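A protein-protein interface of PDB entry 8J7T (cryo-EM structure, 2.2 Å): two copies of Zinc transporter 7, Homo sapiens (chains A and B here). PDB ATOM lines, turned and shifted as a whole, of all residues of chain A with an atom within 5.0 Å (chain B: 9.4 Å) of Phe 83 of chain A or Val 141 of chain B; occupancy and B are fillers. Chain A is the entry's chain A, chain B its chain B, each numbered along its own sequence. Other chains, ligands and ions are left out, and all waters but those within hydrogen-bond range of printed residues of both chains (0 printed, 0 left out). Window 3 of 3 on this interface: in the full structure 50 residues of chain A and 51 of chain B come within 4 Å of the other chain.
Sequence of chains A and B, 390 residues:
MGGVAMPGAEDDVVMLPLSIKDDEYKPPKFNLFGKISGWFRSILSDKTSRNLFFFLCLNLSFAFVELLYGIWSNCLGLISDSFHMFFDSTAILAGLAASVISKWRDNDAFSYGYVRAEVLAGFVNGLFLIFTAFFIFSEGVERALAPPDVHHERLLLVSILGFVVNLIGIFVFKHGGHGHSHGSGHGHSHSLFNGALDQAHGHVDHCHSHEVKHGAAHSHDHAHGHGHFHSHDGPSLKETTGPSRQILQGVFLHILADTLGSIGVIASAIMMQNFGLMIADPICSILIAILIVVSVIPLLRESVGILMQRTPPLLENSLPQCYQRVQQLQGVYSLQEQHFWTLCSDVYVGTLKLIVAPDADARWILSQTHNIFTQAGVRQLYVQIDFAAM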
ATOM      1  N   LEU A  67      23.676 -29.654   5.103  1.00  0.00           N
ATOM      2  CA  LEU A  67      23.888 -29.749   3.660  1.00  0.00           C
ATOM      3  C   LEU A  67      23.694 -31.178   3.169  1.00  0.00           C
ATOM      4  O   LEU A  67      23.058 -31.412   2.131  1.00  0.00           O
ATOM      5  CB  LEU A  67      25.290 -29.251   3.308  1.00  0.00           C
ATOM      6  CG  LEU A  67      25.564 -28.827   1.866  1.00  0.00           C
ATOM      7  CD1 LEU A  67      24.779 -27.585   1.495  1.00  0.00           C
ATOM      8  CD2 LEU A  67      27.050 -28.600   1.667  1.00  0.00           C
ATOM      9  N   ILE A  79      19.187 -26.435   2.375  1.00  0.00           N
ATOM     10  CA  ILE A  79      20.404 -25.942   1.738  1.00  0.00           C
ATOM     11  C   ILE A  79      20.616 -24.467   2.053  1.00  0.00           C
ATOM     12  O   ILE A  79      21.740 -24.032   2.341  1.00  0.00           O
ATOM     13  CB  ILE A  79      20.349 -26.195   0.221  1.00  0.00           C
ATOM     14  CG1 ILE A  79      20.191 -27.688  -0.069  1.00  0.00           C
ATOM     15  CG2 ILE A  79      21.602 -25.665  -0.452  1.00  0.00           C
ATOM     16  CD1 ILE A  79      21.372 -28.521   0.356  1.00  0.00           C
ATOM     17  N   SER A  80      19.545 -23.672   2.000  1.00  0.00           N
ATOM     18  CA  SER A  80      19.668 -22.251   2.315  1.00  0.00           C
ATOM     19  C   SER A  80      20.114 -22.042   3.758  1.00  0.00           C
ATOM     20  O   SER A  80      20.977 -21.198   4.036  1.00  0.00           O
ATOM     21  CB  SER A  80      18.343 -21.540   2.052  1.00  0.00           C
ATOM     22  OG  SER A  80      18.459 -20.148   2.282  1.00  0.00           O
ATOM     23  N   ASP A  81      19.543 -22.807   4.690  1.00  0.00           N
ATOM     24  CA  ASP A  81      19.938 -22.695   6.088  1.00  0.00           C
ATOM     25  C   ASP A  81      21.384 -23.120   6.290  1.00  0.00           C
ATOM     26  O   ASP A  81      22.105 -22.513   7.084  1.00  0.00           O
ATOM     27  CB  ASP A  81      19.005 -23.525   6.966  1.00  0.00           C
ATOM     28  CG  ASP A  81      18.759 -22.887   8.318  1.00  0.00           C
ATOM     29  OD1 ASP A  81      18.110 -21.821   8.364  1.00  0.00           O
ATOM     30  OD2 ASP A  81      19.216 -23.450   9.334  1.00  0.00           O
ATOM     31  N   SER A  82      21.825 -24.168   5.591  1.00  0.00           N
ATOM     32  CA  SER A  82      23.218 -24.588   5.700  1.00  0.00           C
ATOM     33  C   SER A  82      24.165 -23.509   5.188  1.00  0.00           C
ATOM     34  O   SER A  82      25.224 -23.266   5.780  1.00  0.00           O
ATOM     35  CB  SER A  82      23.428 -25.895   4.940  1.00  0.00           C
ATOM     36  OG  SER A  82      23.322 -25.680   3.546  1.00  0.00           O
ATOM     37  N   PHE A  83      23.803 -22.857   4.081  1.00  0.00           N
ATOM     38  CA  PHE A  83      24.633 -21.772   3.566  1.00  0.00           C
ATOM     39  C   PHE A  83      24.685 -20.605   4.544  1.00  0.00           C
ATOM     40  O   PHE A  83      25.754 -20.021   4.778  1.00  0.00           O
ATOM     41  CB  PHE A  83      24.110 -21.319   2.205  1.00  0.00           C
ATOM     42  CG  PHE A  83      24.428 -22.272   1.094  1.00  0.00           C
ATOM     43  CD1 PHE A  83      25.396 -23.246   1.261  1.00  0.00           C
ATOM     44  CD2 PHE A  83      23.747 -22.211  -0.107  1.00  0.00           C
ATOM     45  CE1 PHE A  83      25.689 -24.130   0.247  1.00  0.00           C
ATOM     46  CE2 PHE A  83      24.035 -23.095  -1.125  1.00  0.00           C
ATOM     47  CZ  PHE A  83      25.008 -24.056  -0.947  1.00  0.00           C
ATOM     48  N   HIS A  84      23.542 -20.256   5.136  1.00  0.00           N
ATOM     49  CA  HIS A  84      23.539 -19.202   6.144  1.00  0.00           C
ATOM     50  C   HIS A  84      24.351 -19.598   7.370  1.00  0.00           C
ATOM     51  O   HIS A  84      24.990 -18.745   7.990  1.00  0.00           O
ATOM     52  CB  HIS A  84      22.106 -18.855   6.539  1.00  0.00           C
ATOM     53  CG  HIS A  84      21.409 -17.971   5.553  1.00  0.00           C
ATOM     54  ND1 HIS A  84      20.959 -16.710   5.874  1.00  0.00           N
ATOM     55  CD2 HIS A  84      21.092 -18.165   4.251  1.00  0.00           C
ATOM     56  CE1 HIS A  84      20.390 -16.165   4.813  1.00  0.00           C
ATOM     57  NE2 HIS A  84      20.457 -17.028   3.816  1.00  0.00           N
ATOM     58  N   MET A  85      24.350 -20.882   7.728  1.00  0.00           N
ATOM     59  CA  MET A  85      25.137 -21.331   8.871  1.00  0.00           C
ATOM     60  C   MET A  85      26.628 -21.253   8.582  1.00  0.00           C
ATOM     61  O   MET A  85      27.416 -20.899   9.464  1.00  0.00           O
ATOM     62  CB  MET A  85      24.738 -22.753   9.262  1.00  0.00           C
ATOM     63  CG  MET A  85      23.414 -22.834   9.999  1.00  0.00           C
ATOM     64  SD  MET A  85      23.391 -24.084  11.294  1.00  0.00           S
ATOM     65  CE  MET A  85      25.038 -23.905  11.970  1.00  0.00           C
ATOM     66  N   PHE A  86      27.038 -21.591   7.358  1.00  0.00           N
ATOM     67  CA  PHE A  86      28.437 -21.407   6.980  1.00  0.00           C
ATOM     68  C   PHE A  86      28.825 -19.935   7.035  1.00  0.00           C
ATOM     69  O   PHE A  86      29.897 -19.577   7.549  1.00  0.00           O
ATOM     70  CB  PHE A  86      28.688 -21.970   5.583  1.00  0.00           C
ATOM     71  CG  PHE A  86      28.830 -23.463   5.546  1.00  0.00           C
ATOM     72  CD1 PHE A  86      29.764 -24.101   6.339  1.00  0.00           C
ATOM     73  CD2 PHE A  86      28.036 -24.227   4.711  1.00  0.00           C
ATOM     74  CE1 PHE A  86      29.900 -25.474   6.303  1.00  0.00           C
ATOM     75  CE2 PHE A  86      28.167 -25.599   4.672  1.00  0.00           C
ATOM     76  CZ  PHE A  86      29.100 -26.223   5.469  1.00  0.00           C
ATOM     77  N   PHE A  87      27.952 -19.064   6.529  1.00  0.00           N
ATOM     78  CA  PHE A  87      28.219 -17.632   6.602  1.00  0.00           C
ATOM     79  C   PHE A  87      28.362 -17.174   8.047  1.00  0.00           C
ATOM     80  O   PHE A  87      29.254 -16.385   8.369  1.00  0.00           O
ATOM     81  CB  PHE A  87      27.109 -16.857   5.897  1.00  0.00           C
ATOM     82  CG  PHE A  87      27.448 -15.423   5.640  1.00  0.00           C
ATOM     83  CD1 PHE A  87      28.557 -15.084   4.890  1.00  0.00           C
ATOM     84  CD2 PHE A  87      26.657 -14.412   6.155  1.00  0.00           C
ATOM     85  CE1 PHE A  87      28.872 -13.763   4.653  1.00  0.00           C
ATOM     86  CE2 PHE A  87      26.966 -13.091   5.921  1.00  0.00           C
ATOM     87  CZ  PHE A  87      28.073 -12.767   5.169  1.00  0.00           C
ATOM     88  N   ALA B 133      28.757 -10.938  -2.569  1.00  0.00           N
ATOM     89  CA  ALA B 133      29.281 -11.959  -3.468  1.00  0.00           C
ATOM     90  C   ALA B 133      28.957 -13.353  -2.956  1.00  0.00           C
ATOM     91  O   ALA B 133      28.398 -14.179  -3.688  1.00  0.00           O
ATOM     92  CB  ALA B 133      30.791 -11.782  -3.629  1.00  0.00           C
ATOM     93  N   PHE B 134      29.253 -13.611  -1.681  1.00  0.00           N
ATOM     94  CA  PHE B 134      28.972 -14.922  -1.107  1.00  0.00           C
ATOM     95  C   PHE B 134      27.509 -15.280  -1.303  1.00  0.00           C
ATOM     96  O   PHE B 134      27.185 -16.361  -1.808  1.00  0.00           O
ATOM     97  CB  PHE B 134      29.371 -14.939   0.376  1.00  0.00           C
ATOM     98  CG  PHE B 134      28.884 -16.153   1.150  1.00  0.00           C
ATOM     99  CD1 PHE B 134      27.546 -16.336   1.465  1.00  0.00           C
ATOM    100  CD2 PHE B 134      29.788 -17.128   1.540  1.00  0.00           C
ATOM    101  CE1 PHE B 134      27.124 -17.446   2.154  1.00  0.00           C
ATOM    102  CE2 PHE B 134      29.370 -18.246   2.233  1.00  0.00           C
ATOM    103  CZ  PHE B 134      28.037 -18.405   2.540  1.00  0.00           C
ATOM    104  N   PHE B 135      26.608 -14.363  -0.951  1.00  0.00           N
ATOM    105  CA  PHE B 135      25.192 -14.665  -1.103  1.00  0.00           C
ATOM    106  C   PHE B 135      24.846 -14.893  -2.565  1.00  0.00           C
ATOM    107  O   PHE B 135      24.090 -15.816  -2.889  1.00  0.00           O
ATOM    108  CB  PHE B 135      24.339 -13.557  -0.495  1.00  0.00           C
ATOM    109  CG  PHE B 135      23.971 -13.811   0.936  1.00  0.00           C
ATOM    110  CD1 PHE B 135      24.866 -14.430   1.791  1.00  0.00           C
ATOM    111  CD2 PHE B 135      22.729 -13.448   1.424  1.00  0.00           C
ATOM    112  CE1 PHE B 135      24.538 -14.677   3.108  1.00  0.00           C
ATOM    113  CE2 PHE B 135      22.393 -13.690   2.744  1.00  0.00           C
ATOM    114  CZ  PHE B 135      23.301 -14.307   3.585  1.00  0.00           C
ATOM    115  N   ILE B 136      25.437 -14.103  -3.466  1.00  0.00           N
ATOM    116  CA  ILE B 136      25.278 -14.377  -4.890  1.00  0.00           C
ATOM    117  C   ILE B 136      25.672 -15.817  -5.173  1.00  0.00           C
ATOM    118  O   ILE B 136      24.880 -16.608  -5.701  1.00  0.00           O
ATOM    119  CB  ILE B 136      26.112 -13.391  -5.727  1.00  0.00           C
ATOM    120  CG1 ILE B 136      25.539 -11.979  -5.617  1.00  0.00           C
ATOM    121  CG2 ILE B 136      26.167 -13.837  -7.171  1.00  0.00           C
ATOM    122  CD1 ILE B 136      26.365 -10.937  -6.329  1.00  0.00           C
ATOM    123  N   PHE B 137      26.882 -16.192  -4.743  1.00  0.00           N
ATOM    124  CA  PHE B 137      27.330 -17.574  -4.794  1.00  0.00           C
ATOM    125  C   PHE B 137      26.225 -18.488  -4.295  1.00  0.00           C
ATOM    126  O   PHE B 137      25.719 -19.341  -5.035  1.00  0.00           O
ATOM    127  CB  PHE B 137      28.605 -17.724  -3.950  1.00  0.00           C
ATOM    128  CG  PHE B 137      29.166 -19.119  -3.915  1.00  0.00           C
ATOM    129  CD1 PHE B 137      28.621 -20.090  -3.091  1.00  0.00           C
ATOM    130  CD2 PHE B 137      30.264 -19.451  -4.687  1.00  0.00           C
ATOM    131  CE1 PHE B 137      29.144 -21.366  -3.059  1.00  0.00           C
ATOM    132  CE2 PHE B 137      30.789 -20.725  -4.660  1.00  0.00           C
ATOM    133  CZ  PHE B 137      30.231 -21.683  -3.845  1.00  0.00           C
ATOM    134  N   SER B 138      25.786 -18.247  -3.057  1.00  0.00           N
ATOM    135  CA  SER B 138      24.759 -19.084  -2.452  1.00  0.00           C
ATOM    136  C   SER B 138      23.553 -19.200  -3.367  1.00  0.00           C
ATOM    137  O   SER B 138      23.133 -20.310  -3.720  1.00  0.00           O
ATOM    138  CB  SER B 138      24.355 -18.510  -1.093  1.00  0.00           C
ATOM    139  OG  SER B 138      23.061 -18.952  -0.723  1.00  0.00           O
ATOM    140  N   GLU B 139      23.037 -18.059  -3.831  1.00  0.00           N
ATOM    141  CA  GLU B 139      21.834 -18.086  -4.654  1.00  0.00           C
ATOM    142  C   GLU B 139      22.053 -18.966  -5.871  1.00  0.00           C
ATOM    143  O   GLU B 139      21.240 -19.852  -6.166  1.00  0.00           O
ATOM    144  CB  GLU B 139      21.439 -16.670  -5.072  1.00  0.00           C
ATOM    145  CG  GLU B 139      21.078 -15.743  -3.920  1.00  0.00           C
ATOM    146  CD  GLU B 139      20.596 -16.486  -2.688  1.00  0.00           C
ATOM    147  OE1 GLU B 139      19.392 -16.807  -2.619  1.00  0.00           O
ATOM    148  OE2 GLU B 139      21.420 -16.740  -1.784  1.00  0.00           O
ATOM    149  N   GLY B 140      23.198 -18.794  -6.535  1.00  0.00           N
ATOM    150  CA  GLY B 140      23.468 -19.598  -7.711  1.00  0.00           C
ATOM    151  C   GLY B 140      23.401 -21.076  -7.400  1.00  0.00           C
ATOM    152  O   GLY B 140      22.704 -21.835  -8.078  1.00  0.00           O
ATOM    153  N   VAL B 141      24.052 -21.486  -6.307  1.00  0.00           N
ATOM    154  CA  VAL B 141      24.041 -22.898  -5.946  1.00  0.00           C
ATOM    155  C   VAL B 141      22.612 -23.364  -5.720  1.00  0.00           C
ATOM    156  O   VAL B 141      22.207 -24.429  -6.201  1.00  0.00           O
ATOM    157  CB  VAL B 141      24.927 -23.153  -4.714  1.00  0.00           C
ATOM    158  CG1 VAL B 141      25.030 -24.642  -4.447  1.00  0.00           C
ATOM    159  CG2 VAL B 141      26.303 -22.556  -4.924  1.00  0.00           C
ATOM    160  N   GLU B 142      21.810 -22.551  -5.027  1.00  0.00           N
ATOM    161  CA  GLU B 142      20.418 -22.927  -4.821  1.00  0.00           C
ATOM    162  C   GLU B 142      19.698 -23.060  -6.154  1.00  0.00           C
ATOM    163  O   GLU B 142      18.989 -24.044  -6.389  1.00  0.00           O
ATOM    164  CB  GLU B 142      19.719 -21.908  -3.923  1.00  0.00           C
ATOM    165  CG  GLU B 142      20.266 -21.867  -2.510  1.00  0.00           C
ATOM    166  CD  GLU B 142      19.972 -20.556  -1.811  1.00  0.00           C
ATOM    167  OE1 GLU B 142      19.303 -19.695  -2.417  1.00  0.00           O
ATOM    168  OE2 GLU B 142      20.414 -20.384  -0.654  1.00  0.00           O
ATOM    169  N   ARG B 143      19.919 -22.106  -7.064  1.00  0.00           N
ATOM    170  CA  ARG B 143      19.273 -22.195  -8.365  1.00  0.00           C
ATOM    171  C   ARG B 143      19.786 -23.380  -9.167  1.00  0.00           C
ATOM    172  O   ARG B 143      19.117 -23.810 -10.111  1.00  0.00           O
ATOM    173  CB  ARG B 143      19.466 -20.892  -9.140  1.00  0.00           C
ATOM    174  CG  ARG B 143      18.201 -20.056  -9.230  1.00  0.00           C
ATOM    175  CD  ARG B 143      18.467 -18.684  -9.821  1.00  0.00           C
ATOM    176  NE  ARG B 143      19.824 -18.222  -9.550  1.00  0.00           N
ATOM    177  CZ  ARG B 143      20.140 -17.342  -8.610  1.00  0.00           C
ATOM    178  NH1 ARG B 143      19.217 -16.797  -7.836  1.00  0.00           N
ATOM    179  NH2 ARG B 143      21.415 -17.000  -8.446  1.00  0.00           N
ATOM    180  N   ALA B 144      20.954 -23.917  -8.811  1.00  0.00           N
ATOM    181  CA  ALA B 144      21.414 -25.150  -9.433  1.00  0.00           C
ATOM    182  C   ALA B 144      20.686 -26.361  -8.863  1.00  0.00           C
ATOM    183  O   ALA B 144      20.386 -27.308  -9.599  1.00  0.00           O
ATOM    184  CB  ALA B 144      22.924 -25.302  -9.252  1.00  0.00           C
ATOM    185  N   LEU B 145      20.412 -26.332  -7.560  1.00  0.00           N
ATOM    186  CA  LEU B 145      19.803 -27.512  -6.898  1.00  0.00           C
ATOM    187  C   LEU B 145      18.285 -27.360  -6.891  1.00  0.00           C
ATOM    188  O   LEU B 145      17.655 -27.945  -5.997  1.00  0.00           O
ATOM    189  CB  LEU B 145      20.335 -27.585  -5.466  1.00  0.00           C
ATOM    190  CG  LEU B 145      21.515 -28.526  -5.238  1.00  0.00           C
ATOM    191  CD1 LEU B 145      21.922 -29.218  -6.528  1.00  0.00           C
ATOM    192  CD2 LEU B 145      22.695 -27.780  -4.637  1.00  0.00           C
ATOM    193  N   ALA B 146      17.733 -26.581  -7.829  1.00  0.00           N
ATOM    194  CA  ALA B 146      16.275 -26.312  -7.833  1.00  0.00           C
ATOM    195  C   ALA B 146      15.769 -26.083  -9.257  1.00  0.00           C
ATOM    196  O   ALA B 146      16.490 -25.440 -10.044  1.00  0.00           O
ATOM    197  CB  ALA B 146      15.982 -25.099  -6.990  1.00  0.00           C
ATOM    198  N   PRO B 147      14.560 -26.564  -9.621  1.00  0.00           N
ATOM    199  CA  PRO B 147      13.988 -26.261 -10.930  1.00  0.00           C
ATOM    200  C   PRO B 147      13.785 -24.742 -10.973  1.00  0.00           C
ATOM    201  O   PRO B 147      13.150 -24.218 -10.078  1.00  0.00           O
ATOM    202  CB  PRO B 147      12.641 -26.993 -10.929  1.00  0.00           C
ATOM    203  CG  PRO B 147      12.782 -28.044  -9.848  1.00  0.00           C
ATOM    204  CD  PRO B 147      13.701 -27.428  -8.814  1.00  0.00           C
ATOM    205  N   ASP B 281      23.474 -20.113 -15.576  1.00  0.00           N
ATOM    206  CA  ASP B 281      23.260 -19.235 -14.427  1.00  0.00           C
ATOM    207  C   ASP B 281      24.180 -19.556 -13.253  1.00  0.00           C
ATOM    208  O   ASP B 281      24.819 -18.623 -12.730  1.00  0.00           O
ATOM    209  CB  ASP B 281      21.781 -19.284 -14.025  1.00  0.00           C
ATOM    210  CG  ASP B 281      21.444 -18.344 -12.880  1.00  0.00           C
ATOM    211  OD1 ASP B 281      22.302 -17.530 -12.479  1.00  0.00           O
ATOM    212  OD2 ASP B 281      20.306 -18.423 -12.376  1.00  0.00           O
ATOM    213  N   PRO B 282      24.300 -20.805 -12.782  1.00  0.00           N
ATOM    214  CA  PRO B 282      25.212 -21.048 -11.650  1.00  0.00           C
ATOM    215  C   PRO B 282      26.656 -20.682 -11.942  1.00  0.00           C
ATOM    216  O   PRO B 282      27.304 -20.052 -11.098  1.00  0.00           O
ATOM    217  CB  PRO B 282      25.047 -22.551 -11.380  1.00  0.00           C
ATOM    218  CG  PRO B 282      23.740 -22.907 -11.970  1.00  0.00           C
ATOM    219  CD  PRO B 282      23.576 -22.030 -13.165  1.00  0.00           C
ATOM    220  N   ILE B 283      27.179 -21.048 -13.115  1.00  0.00           N
ATOM    221  CA  ILE B 283      28.575 -20.739 -13.422  1.00  0.00           C
ATOM    222  C   ILE B 283      28.793 -19.236 -13.460  1.00  0.00           C
ATOM    223  O   ILE B 283      29.794 -18.729 -12.936  1.00  0.00           O
ATOM    224  CB  ILE B 283      29.002 -21.403 -14.744  1.00  0.00           C
ATOM    225  CG1 ILE B 283      28.317 -22.755 -14.914  1.00  0.00           C
ATOM    226  CG2 ILE B 283      30.510 -21.556 -14.793  1.00  0.00           C
ATOM    227  CD1 ILE B 283      28.720 -23.485 -16.174  1.00  0.00           C
ATOM    228  N   CYS B 284      27.873 -18.499 -14.084  1.00  0.00           N
ATOM    229  CA  CYS B 284      28.021 -17.049 -14.149  1.00  0.00           C
ATOM    230  C   CYS B 284      27.973 -16.429 -12.758  1.00  0.00           C
ATOM    231  O   CYS B 284      28.762 -15.532 -12.446  1.00  0.00           O
ATOM    232  CB  CYS B 284      26.941 -16.445 -15.046  1.00  0.00           C
ATOM    233  SG  CYS B 284      25.435 -15.958 -14.184  1.00  0.00           S
ATOM    234  N   SER B 285      27.060 -16.901 -11.905  1.00  0.00           N
ATOM    235  CA  SER B 285      26.972 -16.360 -10.552  1.00  0.00           C
ATOM    236  C   SER B 285      28.255 -16.615  -9.768  1.00  0.00           C
ATOM    237  O   SER B 285      28.783 -15.713  -9.105  1.00  0.00           O
ATOM    238  CB  SER B 285      25.770 -16.961  -9.827  1.00  0.00           C
ATOM    239  OG  SER B 285      26.046 -18.288  -9.420  1.00  0.00           O
ATOM    240  N   ILE B 286      28.782 -17.840  -9.843  1.00  0.00           N
ATOM    241  CA  ILE B 286      30.021 -18.149  -9.129  1.00  0.00           C
ATOM    242  C   ILE B 286      31.165 -17.300  -9.662  1.00  0.00           C
ATOM    243  O   ILE B 286      31.987 -16.781  -8.894  1.00  0.00           O
ATOM    244  CB  ILE B 286      30.350 -19.652  -9.219  1.00  0.00           C
ATOM    245  CG1 ILE B 286      29.149 -20.515  -8.832  1.00  0.00           C
ATOM    246  CG2 ILE B 286      31.548 -19.985  -8.348  1.00  0.00           C
ATOM    247  CD1 ILE B 286      28.500 -20.144  -7.529  1.00  0.00           C
ATOM    248  N   ALA B 289      30.898 -13.750  -8.410  1.00  0.00           N
ATOM    249  CA  ALA B 289      31.249 -13.672  -6.992  1.00  0.00           C
ATOM    250  C   ALA B 289      32.762 -13.713  -6.795  1.00  0.00           C
ATOM    251  O   ALA B 289      33.325 -12.929  -6.013  1.00  0.00           O
ATOM    252  CB  ALA B 289      30.574 -14.804  -6.222  1.00  0.00           C
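OG of Ser 138 of chain B is in hydrogen-bond range of OE2 of Glu 139 of chain B (3.0 Å). OG of Ser 138 of chain B is in hydrogen-bond range of OE2 of Glu 142 of chain B (3.0 Å).
Among the printed residues, merely in contact across the chains: Ser 80 of chain A with Glu 142 of chain B (3.5 Å), Phe 83 of chain A with Phe 134 of chain B (3.6 Å), Phe 83 of chain A with Ser 138 of chain B (3.4 Å), Phe 83 of chain A with Val 141 of chain B (3.5 Å), Phe 83 of chain A with Glu 142 of chain B (3.8 Å), His 84 of chain A with Phe 135 of chain B (3.7 Å), Phe 87 of chain A with Phe 134 of chain B (3.8 Å) and Phe 87 of chain A with Phe 135 of chain B (3.7 Å).
No residue of chain B comes within 4 Å of Ser 82 of chain A. Of chain B, only Phe 134 (3.6 Å), Ser 138 (3.4 Å), Val 141 (3.5 Å) and Glu 142 (3.8 Å) come within 4 Å of Phe 83 of chain A. Of the printed residues of chain B, His 84 of chain A touches Phe 135 (3.7 Å). Of the printed residues of chain B, Phe 87 of chain A touches Phe 134 and Phe 135. Of the printed residues of chain A, Phe 135 of chain B touches His 84 (3.7 Å) and Phe 87 (3.7 Å). Of chain A, only Phe 83 (3.5 Å) comes within 4 Å of Val 141 of chain B. Printed residues of chain A within 4 Å of Glu 142 of chain B: Ser 80 (3.5 Å) and Phe 83 (3.8 Å). The nearest printed residue of chain B that does not touch His 84 of chain A is Ser 138 of chain B (5.4 Å).
Of the 10 printed residues of chain A, 4 touch a printed residue of chain B. Hydrophobic or aromatic side chains of chain A that line the printed part of chain B: Phe 83, His 84 and Phe 87. Among the printed residues, no Asp or Glu carboxylate lies within 4 Å of a Lys or Arg side-chain nitrogen of the other chain.
No position is printed for both chains.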
